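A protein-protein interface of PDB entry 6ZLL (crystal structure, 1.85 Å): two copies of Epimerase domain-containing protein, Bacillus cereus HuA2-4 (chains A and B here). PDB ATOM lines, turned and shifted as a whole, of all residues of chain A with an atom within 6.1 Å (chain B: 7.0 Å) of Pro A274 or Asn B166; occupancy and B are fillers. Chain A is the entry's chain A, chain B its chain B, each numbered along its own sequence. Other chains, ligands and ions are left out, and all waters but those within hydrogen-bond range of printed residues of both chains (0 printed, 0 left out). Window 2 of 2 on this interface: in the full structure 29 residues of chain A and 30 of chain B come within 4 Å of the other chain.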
ATOM      1  N   VAL A  87      36.547 -17.918 -29.479  1.00  0.00           N
ATOM      2  CA  VAL A  87      35.227 -17.760 -28.826  1.00  0.00           C
ATOM      3  C   VAL A  87      34.335 -16.893 -29.718  1.00  0.00           C
ATOM      4  O   VAL A  87      33.169 -17.204 -29.864  1.00  0.00           O
ATOM      5  CB  VAL A  87      35.461 -17.130 -27.447  1.00  0.00           C
ATOM      6  CG1 VAL A  87      34.171 -16.675 -26.817  1.00  0.00           C
ATOM      7  CG2 VAL A  87      36.250 -18.056 -26.551  1.00  0.00           C
ATOM      8  N   ARG A  88      34.902 -15.823 -30.274  1.00  0.00           N
ATOM      9  CA  ARG A  88      34.171 -14.713 -30.943  1.00  0.00           C
ATOM     10  C   ARG A  88      33.708 -15.117 -32.357  1.00  0.00           C
ATOM     11  O   ARG A  88      32.748 -14.497 -32.874  1.00  0.00           O
ATOM     12  CB  ARG A  88      35.065 -13.458 -30.909  1.00  0.00           C
ATOM     13  CG  ARG A  88      35.361 -12.946 -29.499  1.00  0.00           C
ATOM     14  CD  ARG A  88      36.203 -11.667 -29.418  1.00  0.00           C
ATOM     15  NE  ARG A  88      37.596 -11.854 -29.815  1.00  0.00           N
ATOM     16  CZ  ARG A  88      38.542 -12.411 -29.065  1.00  0.00           C
ATOM     17  NH1 ARG A  88      39.780 -12.537 -29.524  1.00  0.00           N
ATOM     18  NH2 ARG A  88      38.267 -12.832 -27.839  1.00  0.00           N
ATOM     19  N   TRP A  91      29.872 -18.366 -34.090  1.00  0.00           N
ATOM     20  CA  TRP A  91      28.413 -18.207 -34.333  1.00  0.00           C
ATOM     21  C   TRP A  91      27.996 -18.578 -35.757  1.00  0.00           C
ATOM     22  O   TRP A  91      28.858 -18.602 -36.670  1.00  0.00           O
ATOM     23  CB  TRP A  91      28.045 -16.755 -34.065  1.00  0.00           C
ATOM     24  CG  TRP A  91      28.387 -16.361 -32.671  1.00  0.00           C
ATOM     25  CD1 TRP A  91      29.457 -15.626 -32.280  1.00  0.00           C
ATOM     26  CD2 TRP A  91      27.678 -16.733 -31.477  1.00  0.00           C
ATOM     27  NE1 TRP A  91      29.468 -15.514 -30.918  1.00  0.00           N
ATOM     28  CE2 TRP A  91      28.377 -16.160 -30.397  1.00  0.00           C
ATOM     29  CE3 TRP A  91      26.537 -17.494 -31.220  1.00  0.00           C
ATOM     30  CZ2 TRP A  91      27.945 -16.271 -29.080  1.00  0.00           C
ATOM     31  CZ3 TRP A  91      26.121 -17.628 -29.913  1.00  0.00           C
ATOM     32  CH2 TRP A  91      26.812 -17.021 -28.863  1.00  0.00           C
ATOM     33  N   LEU A 146      29.395 -20.172 -22.325  1.00  0.00           N
ATOM     34  CA  LEU A 146      28.759 -18.944 -22.840  1.00  0.00           C
ATOM     35  C   LEU A 146      28.873 -18.889 -24.363  1.00  0.00           C
ATOM     36  O   LEU A 146      28.246 -17.981 -24.971  1.00  0.00           O
ATOM     37  CB  LEU A 146      29.464 -17.725 -22.230  1.00  0.00           C
ATOM     38  CG  LEU A 146      28.748 -16.965 -21.117  1.00  0.00           C
ATOM     39  CD1 LEU A 146      29.522 -15.679 -20.817  1.00  0.00           C
ATOM     40  CD2 LEU A 146      27.294 -16.637 -21.472  1.00  0.00           C
ATOM     41  N   SER A 147      29.748 -19.677 -24.968  1.00  0.00           N
ATOM     42  CA  SER A 147      30.023 -19.587 -26.427  1.00  0.00           C
ATOM     43  C   SER A 147      29.788 -20.933 -27.088  1.00  0.00           C
ATOM     44  O   SER A 147      30.063 -21.970 -26.482  1.00  0.00           O
ATOM     45  CB  SER A 147      31.438 -19.108 -26.723  1.00  0.00           C
ATOM     46  OG  SER A 147      32.413 -20.073 -26.331  1.00  0.00           O
ATOM     47  N   PRO A 148      29.398 -20.945 -28.379  1.00  0.00           N
ATOM     48  CA  PRO A 148      29.348 -22.183 -29.164  1.00  0.00           C
ATOM     49  C   PRO A 148      30.692 -22.906 -29.143  1.00  0.00           C
ATOM     50  O   PRO A 148      30.704 -24.089 -29.046  1.00  0.00           O
ATOM     51  CB  PRO A 148      28.965 -21.727 -30.574  1.00  0.00           C
ATOM     52  CG  PRO A 148      28.256 -20.411 -30.351  1.00  0.00           C
ATOM     53  CD  PRO A 148      28.933 -19.784 -29.144  1.00  0.00           C
ATOM     54  N   SER A 272      30.778  -4.865 -26.888  1.00  0.00           N
ATOM     55  CA  SER A 272      31.221  -6.207 -26.444  1.00  0.00           C
ATOM     56  C   SER A 272      30.584  -7.253 -27.368  1.00  0.00           C
ATOM     57  O   SER A 272      29.492  -7.025 -27.908  1.00  0.00           O
ATOM     58  CB  SER A 272      30.917  -6.462 -24.995  1.00  0.00           C
ATOM     59  OG  SER A 272      29.536  -6.361 -24.788  1.00  0.00           O
ATOM     60  N   VAL A 273      31.260  -8.371 -27.516  1.00  0.00           N
ATOM     61  CA  VAL A 273      30.876  -9.440 -28.474  1.00  0.00           C
ATOM     62  C   VAL A 273      30.214 -10.532 -27.658  1.00  0.00           C
ATOM     63  O   VAL A 273      30.639 -10.802 -26.540  1.00  0.00           O
ATOM     64  CB  VAL A 273      32.130  -9.924 -29.220  1.00  0.00           C
ATOM     65  CG1 VAL A 273      31.997 -11.346 -29.751  1.00  0.00           C
ATOM     66  CG2 VAL A 273      32.462  -8.954 -30.338  1.00  0.00           C
ATOM     67  N   PRO A 274      29.139 -11.168 -28.155  1.00  0.00           N
ATOM     68  CA  PRO A 274      28.519 -12.244 -27.393  1.00  0.00           C
ATOM     69  C   PRO A 274      29.499 -13.421 -27.225  1.00  0.00           C
ATOM     70  O   PRO A 274      30.299 -13.670 -28.120  1.00  0.00           O
ATOM     71  CB  PRO A 274      27.283 -12.610 -28.231  1.00  0.00           C
ATOM     72  CG  PRO A 274      27.589 -12.100 -29.631  1.00  0.00           C
ATOM     73  CD  PRO A 274      28.449 -10.873 -29.425  1.00  0.00           C
ATOM     74  N   GLY A 275      29.356 -14.133 -26.106  1.00  0.00           N
ATOM     75  CA  GLY A 275      30.004 -15.435 -25.852  1.00  0.00           C
ATOM     76  C   GLY A 275      31.212 -15.322 -24.960  1.00  0.00           C
ATOM     77  O   GLY A 275      31.814 -16.375 -24.647  1.00  0.00           O
ATOM     78  N   GLU A 276      31.555 -14.092 -24.556  1.00  0.00           N
ATOM     79  CA  GLU A 276      32.741 -13.788 -23.716  1.00  0.00           C
ATOM     80  C   GLU A 276      32.330 -13.506 -22.278  1.00  0.00           C
ATOM     81  O   GLU A 276      31.552 -12.605 -22.023  1.00  0.00           O
ATOM     82  CB  GLU A 276      33.478 -12.572 -24.260  1.00  0.00           C
ATOM     83  CG  GLU A 276      33.914 -12.747 -25.698  1.00  0.00           C
ATOM     84  CD  GLU A 276      35.160 -11.960 -25.983  1.00  0.00           C
ATOM     85  OE1 GLU A 276      35.078 -10.714 -25.965  1.00  0.00           O
ATOM     86  OE2 GLU A 276      36.197 -12.597 -26.160  1.00  0.00           O
ATOM     87  N   CYS B 160      21.333 -24.276 -25.853  1.00  0.00           N
ATOM     88  CA  CYS B 160      20.171 -23.486 -25.386  1.00  0.00           C
ATOM     89  C   CYS B 160      20.640 -22.421 -24.387  1.00  0.00           C
ATOM     90  O   CYS B 160      20.166 -21.297 -24.497  1.00  0.00           O
ATOM     91  CB  CYS B 160      19.087 -24.356 -24.767  1.00  0.00           C
ATOM     92  SG  CYS B 160      18.316 -25.395 -26.026  1.00  0.00           S
ATOM     93  N   HIS B 161      21.512 -22.773 -23.451  1.00  0.00           N
ATOM     94  CA  HIS B 161      22.030 -21.860 -22.398  1.00  0.00           C
ATOM     95  C   HIS B 161      22.863 -20.736 -23.028  1.00  0.00           C
ATOM     96  O   HIS B 161      22.771 -19.590 -22.554  1.00  0.00           O
ATOM     97  CB  HIS B 161      22.848 -22.636 -21.368  1.00  0.00           C
ATOM     98  CG  HIS B 161      22.038 -23.540 -20.517  1.00  0.00           C
ATOM     99  ND1 HIS B 161      20.956 -23.082 -19.801  1.00  0.00           N
ATOM    100  CD2 HIS B 161      22.171 -24.859 -20.238  1.00  0.00           C
ATOM    101  CE1 HIS B 161      20.440 -24.093 -19.124  1.00  0.00           C
ATOM    102  NE2 HIS B 161      21.165 -25.194 -19.386  1.00  0.00           N
ATOM    103  N   VAL B 162      23.668 -21.050 -24.040  1.00  0.00           N
ATOM    104  CA  VAL B 162      24.436 -20.031 -24.815  1.00  0.00           C
ATOM    105  C   VAL B 162      23.471 -18.998 -25.411  1.00  0.00           C
ATOM    106  O   VAL B 162      23.756 -17.781 -25.274  1.00  0.00           O
ATOM    107  CB  VAL B 162      25.286 -20.701 -25.903  1.00  0.00           C
ATOM    108  CG1 VAL B 162      25.910 -19.691 -26.861  1.00  0.00           C
ATOM    109  CG2 VAL B 162      26.353 -21.587 -25.255  1.00  0.00           C
ATOM    110  N   TYR B 163      22.413 -19.435 -26.095  1.00  0.00           N
ATOM    111  CA  TYR B 163      21.527 -18.504 -26.845  1.00  0.00           C
ATOM    112  C   TYR B 163      20.581 -17.783 -25.866  1.00  0.00           C
ATOM    113  O   TYR B 163      20.178 -16.621 -26.166  1.00  0.00           O
ATOM    114  CB  TYR B 163      20.878 -19.202 -28.039  1.00  0.00           C
ATOM    115  CG  TYR B 163      21.842 -19.480 -29.165  1.00  0.00           C
ATOM    116  CD1 TYR B 163      22.802 -20.480 -29.065  1.00  0.00           C
ATOM    117  CD2 TYR B 163      21.826 -18.725 -30.325  1.00  0.00           C
ATOM    118  CE1 TYR B 163      23.685 -20.745 -30.103  1.00  0.00           C
ATOM    119  CE2 TYR B 163      22.721 -18.955 -31.360  1.00  0.00           C
ATOM    120  CZ  TYR B 163      23.646 -19.983 -31.257  1.00  0.00           C
ATOM    121  OH  TYR B 163      24.536 -20.178 -32.276  1.00  0.00           O
ATOM    122  N   HIS B 164      20.205 -18.425 -24.756  1.00  0.00           N
ATOM    123  CA  HIS B 164      19.445 -17.777 -23.649  1.00  0.00           C
ATOM    124  C   HIS B 164      20.292 -16.632 -23.069  1.00  0.00           C
ATOM    125  O   HIS B 164      19.815 -15.504 -23.015  1.00  0.00           O
ATOM    126  CB  HIS B 164      19.085 -18.810 -22.578  1.00  0.00           C
ATOM    127  CG  HIS B 164      18.515 -18.227 -21.327  1.00  0.00           C
ATOM    128  ND1 HIS B 164      17.423 -17.357 -21.344  1.00  0.00           N
ATOM    129  CD2 HIS B 164      18.865 -18.377 -20.035  1.00  0.00           C
ATOM    130  CE1 HIS B 164      17.159 -16.984 -20.115  1.00  0.00           C
ATOM    131  NE2 HIS B 164      18.016 -17.592 -19.297  1.00  0.00           N
ATOM    132  N   LYS B 165      21.534 -16.912 -22.690  1.00  0.00           N
ATOM    133  CA  LYS B 165      22.403 -15.939 -21.979  1.00  0.00           C
ATOM    134  C   LYS B 165      22.730 -14.772 -22.920  1.00  0.00           C
ATOM    135  O   LYS B 165      22.690 -13.605 -22.497  1.00  0.00           O
ATOM    136  CB  LYS B 165      23.645 -16.656 -21.445  1.00  0.00           C
ATOM    137  CG  LYS B 165      23.695 -16.905 -19.950  1.00  0.00           C
ATOM    138  CD  LYS B 165      22.479 -17.551 -19.350  1.00  0.00           C
ATOM    139  CE  LYS B 165      22.566 -17.624 -17.835  1.00  0.00           C
ATOM    140  NZ  LYS B 165      22.176 -16.342 -17.196  1.00  0.00           N
ATOM    141  N   ASN B 166      23.002 -15.053 -24.185  1.00  0.00           N
ATOM    142  CA  ASN B 166      23.532 -14.029 -25.111  1.00  0.00           C
ATOM    143  C   ASN B 166      22.397 -13.295 -25.832  1.00  0.00           C
ATOM    144  O   ASN B 166      22.592 -12.120 -26.134  1.00  0.00           O
ATOM    145  CB  ASN B 166      24.505 -14.651 -26.098  1.00  0.00           C
ATOM    146  CG  ASN B 166      25.809 -14.995 -25.424  1.00  0.00           C
ATOM    147  OD1 ASN B 166      26.614 -14.090 -25.183  1.00  0.00           O
ATOM    148  ND2 ASN B 166      26.054 -16.279 -25.172  1.00  0.00           N
ATOM    149  N   PHE B 167      21.277 -13.949 -26.142  1.00  0.00           N
ATOM    150  CA  PHE B 167      20.245 -13.383 -27.044  1.00  0.00           C
ATOM    151  C   PHE B 167      18.861 -13.412 -26.388  1.00  0.00           C
ATOM    152  O   PHE B 167      17.913 -13.005 -27.054  1.00  0.00           O
ATOM    153  CB  PHE B 167      20.255 -14.139 -28.370  1.00  0.00           C
ATOM    154  CG  PHE B 167      21.601 -14.148 -29.027  1.00  0.00           C
ATOM    155  CD1 PHE B 167      22.165 -12.963 -29.480  1.00  0.00           C
ATOM    156  CD2 PHE B 167      22.321 -15.327 -29.153  1.00  0.00           C
ATOM    157  CE1 PHE B 167      23.411 -12.963 -30.088  1.00  0.00           C
ATOM    158  CE2 PHE B 167      23.571 -15.321 -29.750  1.00  0.00           C
ATOM    159  CZ  PHE B 167      24.122 -14.143 -30.206  1.00  0.00           C
ATOM    160  N   HIS B 168      18.787 -13.793 -25.118  1.00  0.00           N
ATOM    161  CA  HIS B 168      17.554 -13.832 -24.302  1.00  0.00           C
ATOM    162  C   HIS B 168      16.516 -14.717 -24.992  1.00  0.00           C
ATOM    163  O   HIS B 168      15.346 -14.403 -24.893  1.00  0.00           O
ATOM    164  CB  HIS B 168      17.078 -12.386 -24.025  1.00  0.00           C
ATOM    165  CG  HIS B 168      18.211 -11.512 -23.583  1.00  0.00           C
ATOM    166  ND1 HIS B 168      18.827 -11.677 -22.360  1.00  0.00           N
ATOM    167  CD2 HIS B 168      18.901 -10.545 -24.225  1.00  0.00           C
ATOM    168  CE1 HIS B 168      19.822 -10.823 -22.249  1.00  0.00           C
ATOM    169  NE2 HIS B 168      19.897 -10.133 -23.383  1.00  0.00           N
ATOM    170  N   ILE B 169      16.913 -15.777 -25.705  1.00  0.00           N
ATOM    171  CA  ILE B 169      15.909 -16.776 -26.180  1.00  0.00           C
ATOM    172  C   ILE B 169      15.298 -17.391 -24.919  1.00  0.00           C
ATOM    173  O   ILE B 169      16.025 -17.803 -24.025  1.00  0.00           O
ATOM    174  CB  ILE B 169      16.503 -17.800 -27.155  1.00  0.00           C
ATOM    175  CG1 ILE B 169      17.002 -17.120 -28.442  1.00  0.00           C
ATOM    176  CG2 ILE B 169      15.519 -18.916 -27.455  1.00  0.00           C
ATOM    177  CD1 ILE B 169      17.588 -18.085 -29.460  1.00  0.00           C
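O of Leu A146 is in hydrogen-bond range of ND2 of Asn B166 (2.8 Å).
The backbone NH (N) of Gly A275 lies within hydrogen-bond range of the side-chain amide oxygen (OD1) of Asn B166.
NE1 of Trp A91 lies within hydrogen-bond range of O of Pro A274.
The side-chain amide nitrogen (ND2) of Asn B166 lies within hydrogen-bond range of the backbone carbonyl oxygen (O) of Val B162, at 2.7 Å.
The backbone carbonyl oxygen (O) of Tyr B163 is in hydrogen-bond range of the backbone NH (N) of His B168 (3.3 Å).
The backbone NH (N) of Ile B169 sits at hydrogen-bond distance from the backbone carbonyl oxygen (O) of Tyr B163, 3.4 Å away.
Among the printed residues, pairs that only touch across the chains: Trp A91 with Val B162, Trp A91 with Tyr B163, Trp A91 with Asn B166, Trp A91 with Phe B167, Leu A146 with Val B162, Leu A146 with Lys B165, Ser A147 with Val B162, Pro A148 with Val B162 and Pro A274 with Asn B166.
Asn B166 touches just these residues of chain A: Trp A91 (3.8 Å), Leu A146 (2.8 Å), Pro A274 (3.5 Å) and Gly A275 (2.9 Å).
Of the printed residues of chain B, Leu A146 touches Val B162 (3.5 Å), Lys B165 (3.6 Å) and Asn B166 (2.8 Å).
Printed residues of chain B within 4 Å of Ser A147: Val B162.
Printed residues of chain A within 4 Å of Tyr B163: Trp A91 (3.5 Å).
Printed residues of chain B within 4 Å of Gly A275: Asn B166.
The nearest residue of chain B that does not touch Pro A274 is Phe B167 (4.03 Å).
Printed residues of chain B that touch a printed residue of chain A: Val B162, Tyr B163, Lys B165, Asn B166 and Phe B167.
Hydrophobic or aromatic side chains of chain B within 4 Å of the printed part of chain A: Val B162, Tyr B163 and Phe B167.
Of the 11 printed residues of chain A, 6 touch a printed residue of chain B.
Hydrophobic or aromatic side chains of chain A that line the printed part of chain B: Trp A91, Leu A146, Pro A148 and Pro A274.
Along chain A the printed residues that touch a printed residue of chain B span positions 91 to 275.
Among the printed residues, no Asp or Glu carboxylate lies within 4 Å of a Lys or Arg side-chain nitrogen of the other chain.
No position is printed for both chains.
Of the 11 pairs that touch across the chains among the printed residues, none has its exchanged pair printed and touching as well.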
